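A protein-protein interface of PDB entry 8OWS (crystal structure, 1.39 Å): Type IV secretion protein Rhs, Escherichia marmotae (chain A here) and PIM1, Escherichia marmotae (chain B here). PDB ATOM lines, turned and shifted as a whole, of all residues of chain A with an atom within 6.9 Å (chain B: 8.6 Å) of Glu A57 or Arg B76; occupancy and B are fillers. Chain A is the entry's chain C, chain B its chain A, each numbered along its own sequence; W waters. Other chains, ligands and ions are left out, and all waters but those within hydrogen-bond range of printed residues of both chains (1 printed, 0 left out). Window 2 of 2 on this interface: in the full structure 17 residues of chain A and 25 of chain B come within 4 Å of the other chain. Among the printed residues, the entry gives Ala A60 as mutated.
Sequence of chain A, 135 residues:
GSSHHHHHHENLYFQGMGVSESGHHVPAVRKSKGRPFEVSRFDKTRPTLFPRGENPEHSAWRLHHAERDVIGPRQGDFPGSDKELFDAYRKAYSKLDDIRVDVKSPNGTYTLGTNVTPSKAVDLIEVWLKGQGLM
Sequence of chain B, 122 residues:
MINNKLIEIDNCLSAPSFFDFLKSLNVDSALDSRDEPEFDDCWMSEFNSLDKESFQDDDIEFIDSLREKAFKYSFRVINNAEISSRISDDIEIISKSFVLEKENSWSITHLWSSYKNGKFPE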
ATOM      1  N   PRO A  51      -8.720 -25.693  32.027  1.00  0.00           N
ATOM      2  CA  PRO A  51      -9.488 -26.111  33.208  1.00  0.00           C
ATOM      3  C   PRO A  51      -9.577 -27.626  33.317  1.00  0.00           C
ATOM      4  O   PRO A  51      -9.812 -28.329  32.333  1.00  0.00           O
ATOM      5  CB  PRO A  51     -10.873 -25.491  32.975  1.00  0.00           C
ATOM      6  CG  PRO A  51     -10.980 -25.307  31.496  1.00  0.00           C
ATOM      7  CD  PRO A  51      -9.565 -25.067  30.990  1.00  0.00           C
ATOM      8  N   GLU A  54     -14.475 -32.162  36.414  1.00  0.00           N
ATOM      9  CA  GLU A  54     -15.805 -32.215  35.847  1.00  0.00           C
ATOM     10  C   GLU A  54     -16.338 -30.789  35.666  1.00  0.00           C
ATOM     11  O   GLU A  54     -15.999 -29.868  36.424  1.00  0.00           O
ATOM     12  CB  GLU A  54     -16.722 -33.125  36.690  1.00  0.00           C
ATOM     13  CG  GLU A  54     -16.342 -34.637  36.592  1.00  0.00           C
ATOM     14  CD  GLU A  54     -17.130 -35.601  37.521  1.00  0.00           C
ATOM     15  OE1 GLU A  54     -17.473 -35.225  38.680  1.00  0.00           O
ATOM     16  OE2 GLU A  54     -17.382 -36.765  37.082  1.00  0.00           O
ATOM     17  N   ASN A  55     -17.106 -30.607  34.612  1.00  0.00           N
ATOM     18  CA  ASN A  55     -17.794 -29.358  34.312  1.00  0.00           C
ATOM     19  C   ASN A  55     -16.804 -28.218  34.094  1.00  0.00           C
ATOM     20  O   ASN A  55     -16.875 -27.183  34.774  1.00  0.00           O
ATOM     21  CB  ASN A  55     -18.803 -29.025  35.414  1.00  0.00           C
ATOM     22  CG  ASN A  55     -19.880 -28.081  34.939  1.00  0.00           C
ATOM     23  OD1 ASN A  55     -19.963 -27.780  33.754  1.00  0.00           O
ATOM     24  ND2 ASN A  55     -20.710 -27.612  35.855  1.00  0.00           N
ATOM     25  N   PRO A  56     -15.869 -28.368  33.152  1.00  0.00           N
ATOM     26  CA  PRO A  56     -14.936 -27.264  32.875  1.00  0.00           C
ATOM     27  C   PRO A  56     -15.606 -25.980  32.460  1.00  0.00           C
ATOM     28  O   PRO A  56     -15.032 -24.914  32.708  1.00  0.00           O
ATOM     29  CB  PRO A  56     -14.049 -27.826  31.753  1.00  0.00           C
ATOM     30  CG  PRO A  56     -14.836 -28.933  31.162  1.00  0.00           C
ATOM     31  CD  PRO A  56     -15.577 -29.539  32.308  1.00  0.00           C
ATOM     32  N   GLU A  57     -16.784 -26.024  31.828  1.00  0.00           N
ATOM     33  CA  GLU A  57     -17.461 -24.786  31.462  1.00  0.00           C
ATOM     34  C   GLU A  57     -17.736 -23.927  32.687  1.00  0.00           C
ATOM     35  O   GLU A  57     -17.720 -22.694  32.600  1.00  0.00           O
ATOM     36  CB  GLU A  57     -18.767 -25.057  30.707  1.00  0.00           C
ATOM     37  CG  GLU A  57     -19.922 -25.485  31.589  1.00  0.00           C
ATOM     38  CD  GLU A  57     -21.183 -25.804  30.808  1.00  0.00           C
ATOM     39  OE1 GLU A  57     -22.272 -25.738  31.421  1.00  0.00           O
ATOM     40  OE2 GLU A  57     -21.076 -26.099  29.604  1.00  0.00           O
ATOM     41  N   HIS A  58     -17.995 -24.552  33.836  1.00  0.00           N
ATOM     42  CA  HIS A  58     -18.276 -23.766  35.023  1.00  0.00           C
ATOM     43  C   HIS A  58     -17.008 -23.161  35.604  1.00  0.00           C
ATOM     44  O   HIS A  58     -17.022 -22.013  36.052  1.00  0.00           O
ATOM     45  CB  HIS A  58     -19.027 -24.594  36.053  1.00  0.00           C
ATOM     46  CG  HIS A  58     -19.537 -23.778  37.183  1.00  0.00           C
ATOM     47  ND1 HIS A  58     -20.452 -22.755  37.024  1.00  0.00           N
ATOM     48  CD2 HIS A  58     -19.206 -23.789  38.497  1.00  0.00           C
ATOM     49  CE1 HIS A  58     -20.676 -22.190  38.198  1.00  0.00           C
ATOM     50  NE2 HIS A  58     -19.930 -22.799  39.106  1.00  0.00           N
ATOM     51  N   SER A  59     -15.903 -23.909  35.606  1.00  0.00           N
ATOM     52  CA  SER A  59     -14.639 -23.315  36.017  1.00  0.00           C
ATOM     53  C   SER A  59     -14.276 -22.168  35.093  1.00  0.00           C
ATOM     54  O   SER A  59     -13.842 -21.106  35.552  1.00  0.00           O
ATOM     55  CB  SER A  59     -13.554 -24.377  36.015  1.00  0.00           C
ATOM     56  OG  SER A  59     -13.763 -25.273  37.100  1.00  0.00           O
ATOM     57  N   ALA A  60     -14.453 -22.355  33.787  1.00  0.00           N
ATOM     58  CA  ALA A  60     -14.163 -21.300  32.822  1.00  0.00           C
ATOM     59  C   ALA A  60     -15.042 -20.087  33.073  1.00  0.00           C
ATOM     60  O   ALA A  60     -14.558 -18.944  33.049  1.00  0.00           O
ATOM     61  CB  ALA A  60     -14.354 -21.834  31.403  1.00  0.00           C
ATOM     62  N   TRP A  61     -16.335 -20.310  33.337  1.00  0.00           N
ATOM     63  CA  TRP A  61     -17.248 -19.209  33.637  1.00  0.00           C
ATOM     64  C   TRP A  61     -16.845 -18.475  34.914  1.00  0.00           C
ATOM     65  O   TRP A  61     -16.885 -17.244  34.971  1.00  0.00           O
ATOM     66  CB  TRP A  61     -18.682 -19.756  33.742  1.00  0.00           C
ATOM     67  CG  TRP A  61     -19.629 -18.858  34.450  1.00  0.00           C
ATOM     68  CD1 TRP A  61     -20.179 -19.060  35.688  1.00  0.00           C
ATOM     69  CD2 TRP A  61     -20.126 -17.588  33.993  1.00  0.00           C
ATOM     70  NE1 TRP A  61     -20.996 -18.001  36.023  1.00  0.00           N
ATOM     71  CE2 TRP A  61     -20.980 -17.086  34.998  1.00  0.00           C
ATOM     72  CE3 TRP A  61     -19.943 -16.825  32.825  1.00  0.00           C
ATOM     73  CZ2 TRP A  61     -21.645 -15.864  34.878  1.00  0.00           C
ATOM     74  CZ3 TRP A  61     -20.607 -15.613  32.710  1.00  0.00           C
ATOM     75  CH2 TRP A  61     -21.445 -15.144  33.731  1.00  0.00           C
ATOM     76  N   ARG A  62     -16.460 -19.213  35.953  1.00  0.00           N
ATOM     77  CA  ARG A  62     -16.047 -18.581  37.199  1.00  0.00           C
ATOM     78  C   ARG A  62     -14.798 -17.734  36.989  1.00  0.00           C
ATOM     79  O   ARG A  62     -14.683 -16.642  37.549  1.00  0.00           O
ATOM     80  CB  ARG A  62     -15.780 -19.635  38.270  1.00  0.00           C
ATOM     81  CG  ARG A  62     -17.065 -20.266  38.815  1.00  0.00           C
ATOM     82  CD  ARG A  62     -16.755 -21.398  39.754  1.00  0.00           C
ATOM     83  NE  ARG A  62     -16.167 -20.924  41.005  1.00  0.00           N
ATOM     84  CZ  ARG A  62     -15.549 -21.699  41.886  1.00  0.00           C
ATOM     85  NH1 ARG A  62     -15.397 -22.989  41.653  1.00  0.00           N
ATOM     86  NH2 ARG A  62     -15.067 -21.174  42.995  1.00  0.00           N
ATOM     87  N   PHE B  19     -25.277 -21.396  18.697  1.00  0.00           N
ATOM     88  CA  PHE B  19     -23.849 -21.115  18.632  1.00  0.00           C
ATOM     89  C   PHE B  19     -23.076 -22.105  17.766  1.00  0.00           C
ATOM     90  O   PHE B  19     -21.835 -22.084  17.765  1.00  0.00           O
ATOM     91  CB  PHE B  19     -23.253 -21.079  20.048  1.00  0.00           C
ATOM     92  CG  PHE B  19     -23.585 -19.819  20.798  1.00  0.00           C
ATOM     93  CD1 PHE B  19     -24.406 -19.853  21.922  1.00  0.00           C
ATOM     94  CD2 PHE B  19     -23.119 -18.580  20.360  1.00  0.00           C
ATOM     95  CE1 PHE B  19     -24.730 -18.677  22.599  1.00  0.00           C
ATOM     96  CE2 PHE B  19     -23.446 -17.426  21.032  1.00  0.00           C
ATOM     97  CZ  PHE B  19     -24.246 -17.475  22.162  1.00  0.00           C
ATOM     98  N   ASP B  20     -23.778 -22.971  17.024  1.00  0.00           N
ATOM     99  CA  ASP B  20     -23.077 -23.979  16.236  1.00  0.00           C
ATOM    100  C   ASP B  20     -22.169 -23.354  15.178  1.00  0.00           C
ATOM    101  O   ASP B  20     -21.177 -23.980  14.776  1.00  0.00           O
ATOM    102  CB  ASP B  20     -24.074 -24.950  15.580  1.00  0.00           C
ATOM    103  CG  ASP B  20     -24.554 -26.031  16.542  1.00  0.00           C
ATOM    104  OD1 ASP B  20     -24.305 -25.908  17.758  1.00  0.00           O
ATOM    105  OD2 ASP B  20     -25.173 -27.014  16.076  1.00  0.00           O
ATOM    106  N   LEU B  22     -19.927 -21.386  15.539  1.00  0.00           N
ATOM    107  CA  LEU B  22     -18.564 -21.260  16.036  1.00  0.00           C
ATOM    108  C   LEU B  22     -17.660 -22.375  15.545  1.00  0.00           C
ATOM    109  O   LEU B  22     -16.438 -22.220  15.584  1.00  0.00           O
ATOM    110  CB  LEU B  22     -18.571 -21.201  17.565  1.00  0.00           C
ATOM    111  CG  LEU B  22     -19.175 -19.934  18.170  1.00  0.00           C
ATOM    112  CD1 LEU B  22     -19.270 -20.142  19.680  1.00  0.00           C
ATOM    113  CD2 LEU B  22     -18.343 -18.702  17.847  1.00  0.00           C
ATOM    114  N   LYS B  23     -18.226 -23.495  15.094  1.00  0.00           N
ATOM    115  CA  LYS B  23     -17.398 -24.578  14.588  1.00  0.00           C
ATOM    116  C   LYS B  23     -16.600 -24.162  13.357  1.00  0.00           C
ATOM    117  O   LYS B  23     -15.569 -24.776  13.075  1.00  0.00           O
ATOM    118  CB  LYS B  23     -18.280 -25.791  14.259  1.00  0.00           C
ATOM    119  CG  LYS B  23     -18.938 -26.454  15.465  1.00  0.00           C
ATOM    120  CD  LYS B  23     -19.743 -27.694  15.063  1.00  0.00           C
ATOM    121  CE  LYS B  23     -20.751 -28.076  16.154  1.00  0.00           C
ATOM    122  NZ  LYS B  23     -21.450 -29.372  15.899  1.00  0.00           N
ATOM    123  N   GLU B  68     -24.208 -15.755  31.594  1.00  0.00           N
ATOM    124  CA  GLU B  68     -23.824 -17.129  31.912  1.00  0.00           C
ATOM    125  C   GLU B  68     -24.265 -18.080  30.810  1.00  0.00           C
ATOM    126  O   GLU B  68     -23.506 -18.968  30.410  1.00  0.00           O
ATOM    127  CB  GLU B  68     -24.384 -17.549  33.278  1.00  0.00           C
ATOM    128  CG  GLU B  68     -23.934 -18.936  33.689  1.00  0.00           C
ATOM    129  CD  GLU B  68     -24.257 -19.287  35.135  1.00  0.00           C
ATOM    130  OE1 GLU B  68     -24.878 -18.464  35.823  1.00  0.00           O
ATOM    131  OE2 GLU B  68     -23.870 -20.388  35.554  1.00  0.00           O
ATOM    132  N   LYS B  69     -25.483 -17.903  30.296  1.00  0.00           N
ATOM    133  CA  LYS B  69     -25.959 -18.710  29.181  1.00  0.00           C
ATOM    134  C   LYS B  69     -25.096 -18.504  27.944  1.00  0.00           C
ATOM    135  O   LYS B  69     -24.661 -19.470  27.312  1.00  0.00           O
ATOM    136  CB  LYS B  69     -27.418 -18.343  28.885  1.00  0.00           C
ATOM    137  CG  LYS B  69     -28.406 -18.973  29.849  1.00  0.00           C
ATOM    138  CD  LYS B  69     -29.824 -18.449  29.709  1.00  0.00           C
ATOM    139  CE  LYS B  69     -30.757 -19.216  30.643  1.00  0.00           C
ATOM    140  NZ  LYS B  69     -32.130 -18.648  30.690  1.00  0.00           N
ATOM    141  N   ALA B  70     -24.836 -17.255  27.586  1.00  0.00           N
ATOM    142  CA  ALA B  70     -24.022 -16.998  26.406  1.00  0.00           C
ATOM    143  C   ALA B  70     -22.644 -17.616  26.559  1.00  0.00           C
ATOM    144  O   ALA B  70     -22.099 -18.199  25.606  1.00  0.00           O
ATOM    145  CB  ALA B  70     -23.933 -15.499  26.164  1.00  0.00           C
ATOM    146  N   PHE B  71     -22.043 -17.458  27.738  1.00  0.00           N
ATOM    147  CA  PHE B  71     -20.718 -18.026  27.955  1.00  0.00           C
ATOM    148  C   PHE B  71     -20.749 -19.541  27.800  1.00  0.00           C
ATOM    149  O   PHE B  71     -19.959 -20.128  27.043  1.00  0.00           O
ATOM    150  CB  PHE B  71     -20.197 -17.646  29.338  1.00  0.00           C
ATOM    151  CG  PHE B  71     -18.773 -18.070  29.555  1.00  0.00           C
ATOM    152  CD1 PHE B  71     -17.728 -17.177  29.354  1.00  0.00           C
ATOM    153  CD2 PHE B  71     -18.467 -19.377  29.895  1.00  0.00           C
ATOM    154  CE1 PHE B  71     -16.408 -17.588  29.484  1.00  0.00           C
ATOM    155  CE2 PHE B  71     -17.151 -19.792  30.034  1.00  0.00           C
ATOM    156  CZ  PHE B  71     -16.120 -18.884  29.845  1.00  0.00           C
ATOM    157  N   LYS B  72     -21.628 -20.199  28.548  1.00  0.00           N
ATOM    158  CA  LYS B  72     -21.579 -21.653  28.623  1.00  0.00           C
ATOM    159  C   LYS B  72     -22.090 -22.308  27.353  1.00  0.00           C
ATOM    160  O   LYS B  72     -21.493 -23.275  26.884  1.00  0.00           O
ATOM    161  CB  LYS B  72     -22.336 -22.137  29.849  1.00  0.00           C
ATOM    162  CG  LYS B  72     -21.659 -21.743  31.144  1.00  0.00           C
ATOM    163  CD  LYS B  72     -22.398 -22.267  32.355  1.00  0.00           C
ATOM    164  CE  LYS B  72     -21.574 -22.051  33.599  1.00  0.00           C
ATOM    165  NZ  LYS B  72     -22.316 -22.474  34.788  1.00  0.00           N
ATOM    166  N   TYR B  73     -23.158 -21.779  26.760  1.00  0.00           N
ATOM    167  CA  TYR B  73     -23.675 -22.380  25.530  1.00  0.00           C
ATOM    168  C   TYR B  73     -22.640 -22.269  24.410  1.00  0.00           C
ATOM    169  O   TYR B  73     -22.462 -23.194  23.609  1.00  0.00           O
ATOM    170  CB  TYR B  73     -25.027 -21.770  25.144  1.00  0.00           C
ATOM    171  CG  TYR B  73     -26.162 -21.997  26.146  1.00  0.00           C
ATOM    172  CD1 TYR B  73     -27.320 -21.222  26.088  1.00  0.00           C
ATOM    173  CD2 TYR B  73     -26.080 -22.955  27.140  1.00  0.00           C
ATOM    174  CE1 TYR B  73     -28.365 -21.410  26.992  1.00  0.00           C
ATOM    175  CE2 TYR B  73     -27.124 -23.145  28.032  1.00  0.00           C
ATOM    176  CZ  TYR B  73     -28.250 -22.377  27.955  1.00  0.00           C
ATOM    177  OH  TYR B  73     -29.265 -22.587  28.876  1.00  0.00           O
ATOM    178  N   SER B  74     -21.920 -21.147  24.334  1.00  0.00           N
ATOM    179  CA  SER B  74     -20.870 -21.039  23.327  1.00  0.00           C
ATOM    180  C   SER B  74     -19.649 -21.887  23.679  1.00  0.00           C
ATOM    181  O   SER B  74     -18.996 -22.435  22.774  1.00  0.00           O
ATOM    182  CB  SER B  74     -20.497 -19.574  23.117  1.00  0.00           C
ATOM    183  OG  SER B  74     -19.867 -19.003  24.269  1.00  0.00           O
ATOM    184  N   PHE B  75     -19.332 -22.019  24.967  1.00  0.00           N
ATOM    185  CA  PHE B  75     -18.187 -22.825  25.381  1.00  0.00           C
ATOM    186  C   PHE B  75     -18.381 -24.283  25.002  1.00  0.00           C
ATOM    187  O   PHE B  75     -17.413 -24.975  24.677  1.00  0.00           O
ATOM    188  CB  PHE B  75     -17.999 -22.709  26.893  1.00  0.00           C
ATOM    189  CG  PHE B  75     -16.693 -23.279  27.383  1.00  0.00           C
ATOM    190  CD1 PHE B  75     -15.538 -22.513  27.351  1.00  0.00           C
ATOM    191  CD2 PHE B  75     -16.617 -24.572  27.863  1.00  0.00           C
ATOM    192  CE1 PHE B  75     -14.322 -23.030  27.802  1.00  0.00           C
ATOM    193  CE2 PHE B  75     -15.402 -25.087  28.312  1.00  0.00           C
ATOM    194  CZ  PHE B  75     -14.261 -24.303  28.277  1.00  0.00           C
ATOM    195  N   ARG B  76     -19.626 -24.762  25.035  1.00  0.00           N
ATOM    196  CA  ARG B  76     -19.916 -26.145  24.682  1.00  0.00           C
ATOM    197  C   ARG B  76     -19.599 -26.452  23.231  1.00  0.00           C
ATOM    198  O   ARG B  76     -19.351 -27.616  22.902  1.00  0.00           O
ATOM    199  CB  ARG B  76     -21.387 -26.441  24.975  1.00  0.00           C
ATOM    200  CG  ARG B  76     -21.673 -26.479  26.440  1.00  0.00           C
ATOM    201  CD  ARG B  76     -23.164 -26.531  26.712  1.00  0.00           C
ATOM    202  NE  ARG B  76     -23.418 -26.347  28.136  1.00  0.00           N
ATOM    203  CZ  ARG B  76     -24.621 -26.350  28.705  1.00  0.00           C
ATOM    204  NH1 ARG B  76     -24.722 -26.176  30.002  1.00  0.00           N
ATOM    205  NH2 ARG B  76     -25.721 -26.510  27.977  1.00  0.00           N
ATOM    206  N   VAL B  77     -19.561 -25.440  22.366  1.00  0.00           N
ATOM    207  CA  VAL B  77     -19.346 -25.693  20.945  1.00  0.00           C
ATOM    208  C   VAL B  77     -17.861 -25.842  20.629  1.00  0.00           C
ATOM    209  O   VAL B  77     -17.460 -26.798  19.959  1.00  0.00           O
ATOM    210  CB  VAL B  77     -20.019 -24.605  20.087  1.00  0.00           C
ATOM    211  CG1 VAL B  77     -19.887 -24.951  18.588  1.00  0.00           C
ATOM    212  CG2 VAL B  77     -21.490 -24.457  20.461  1.00  0.00           C
ATOM    213  N   ILE B  78     -17.016 -24.905  21.076  1.00  0.00           N
ATOM    214  CA  ILE B  78     -15.598 -24.933  20.733  1.00  0.00           C
ATOM    215  C   ILE B  78     -14.667 -24.810  21.933  1.00  0.00           C
ATOM    216  O   ILE B  78     -13.446 -24.803  21.751  1.00  0.00           O
ATOM    217  CB  ILE B  78     -15.216 -23.912  19.638  1.00  0.00           C
ATOM    218  CG1 ILE B  78     -15.514 -22.477  20.092  1.00  0.00           C
ATOM    219  CG2 ILE B  78     -15.927 -24.232  18.317  1.00  0.00           C
ATOM    220  CD1 ILE B  78     -14.780 -21.434  19.275  1.00  0.00           C
ATOM    221  N   ASN B  79     -15.181 -24.734  23.166  1.00  0.00           N
ATOM    222  CA  ASN B  79     -14.335 -24.839  24.350  1.00  0.00           C
ATOM    223  C   ASN B  79     -13.199 -23.816  24.329  1.00  0.00           C
ATOM    224  O   ASN B  79     -12.049 -24.106  24.681  1.00  0.00           O
ATOM    225  CB  ASN B  79     -13.793 -26.264  24.512  1.00  0.00           C
ATOM    226  CG  ASN B  79     -14.890 -27.296  24.660  1.00  0.00           C
ATOM    227  OD1 ASN B  79     -15.734 -27.208  25.554  1.00  0.00           O
ATOM    228  ND2 ASN B  79     -14.898 -28.280  23.764  1.00  0.00           N
ATOM    229  N   ASN B  80     -13.510 -22.594  23.910  1.00  0.00           N
ATOM    230  CA  ASN B  80     -12.521 -21.528  23.865  1.00  0.00           C
ATOM    231  C   ASN B  80     -12.927 -20.438  24.846  1.00  0.00           C
ATOM    232  O   ASN B  80     -13.960 -19.783  24.660  1.00  0.00           O
ATOM    233  CB  ASN B  80     -12.350 -20.952  22.460  1.00  0.00           C
ATOM    234  CG  ASN B  80     -11.179 -19.998  22.379  1.00  0.00           C
ATOM    235  OD1 ASN B  80     -11.220 -18.907  22.937  1.00  0.00           O
ATOM    236  ND2 ASN B  80     -10.116 -20.410  21.698  1.00  0.00           N
ATOM    237  N   ALA B  81     -12.113 -20.235  25.885  1.00  0.00           N
ATOM    238  CA  ALA B  81     -12.500 -19.304  26.942  1.00  0.00           C
ATOM    239  C   ALA B  81     -12.561 -17.860  26.460  1.00  0.00           C
ATOM    240  O   ALA B  81     -13.462 -17.107  26.855  1.00  0.00           O
ATOM    241  CB  ALA B  81     -11.528 -19.439  28.114  1.00  0.00           C
ATOM    242  N   SER B  84     -15.741 -17.367  24.401  1.00  0.00           N
ATOM    243  CA  SER B  84     -16.918 -17.370  25.271  1.00  0.00           C
ATOM    244  C   SER B  84     -16.975 -16.117  26.140  1.00  0.00           C
ATOM    245  O   SER B  84     -18.057 -15.554  26.365  1.00  0.00           O
ATOM    246  CB  SER B  84     -16.959 -18.641  26.112  1.00  0.00           C
ATOM    247  OG  SER B  84     -17.246 -19.761  25.261  1.00  0.00           O
HETATM  248  O   HOH W   1     -22.475 -25.419  34.081  1.00  0.00           O
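NZ of Lys B72 lies within hydrogen-bond range of ND1 of His A58 (2.9 Å). NE of Arg B76 lies within salt-bridge range of OE2 of Glu A57, at 2.8 Å.
Of the 10 printed residues of chain A, 4 touch a printed residue of chain B. Among the printed residues, Asp or Glu carboxylates within 4 Å of a Lys or Arg side-chain nitrogen of the other chain: Glu A57 with Arg B76 (2.8 Å).
Water W1 lies within hydrogen-bond range of the side-chain carboxylate (OE1) of Glu A57 (2.7 Å), the side-chain amino group (NZ) of Lys B72 (3.0 Å) and the side-chain amide nitrogen (ND2) of Asn A55 (3.3 Å).
Of chain A, only Glu A57 comes within 4 Å of Arg B76. No residue of chain B comes within 4 Å of Pro A56. Of the printed residues of chain A, Glu B68 touches Trp A61 (3.5 Å). Of the printed residues of chain A, Phe B75 touches Glu A57 (3.6 Å) and Ala A60 (3.8 Å). Printed residues of chain B within 4 Å of His A58: Lys B72. Of the printed residues of chain B, Trp A61 touches Glu B68 (3.5 Å), Phe B71 (3.4 Å) and Lys B72 (3.7 Å). Of the printed residues of chain A, Phe B71 touches Glu A57 (3.9 Å), Ala A60 (3.6 Å) and Trp A61 (3.4 Å). Lys B23 touches none of the printed residues of chain A. Phe B19 touches none of the printed residues of chain A. The nearest printed residue of chain B that does not touch Trp A61 is Lys B69 (5.9 Å).
Among the printed residues, merely in contact across the chains: Trp A61 with Phe B71, Trp A61 with Glu B68, Ala A60 with Phe B71, Glu A57 with Lys B72, Glu A57 with Phe B75, Trp A61 with Lys B72, Ala A60 with Phe B75 and Glu A57 with Phe B71.
OE2 of Glu B68 is in salt-bridge range of NZ of Lys B72 (2.7 Å). The backbone carbonyl oxygen (O) of Phe B71 lies within hydrogen-bond range of the side-chain hydroxyl (OG) of Ser B74 (3.0 Å). The backbone carbonyl oxygen (O) of Phe B71 lies within hydrogen-bond range of the side-chain hydroxyl (OG) of Ser B84. The side-chain amide oxygen (OD1) of Asn B79 lies close to the backbone carbonyl oxygen (O) of Phe B75 (2.9 Å). N of Phe B75 is in hydrogen-bond range of OG of Ser B84 (3.1 Å).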
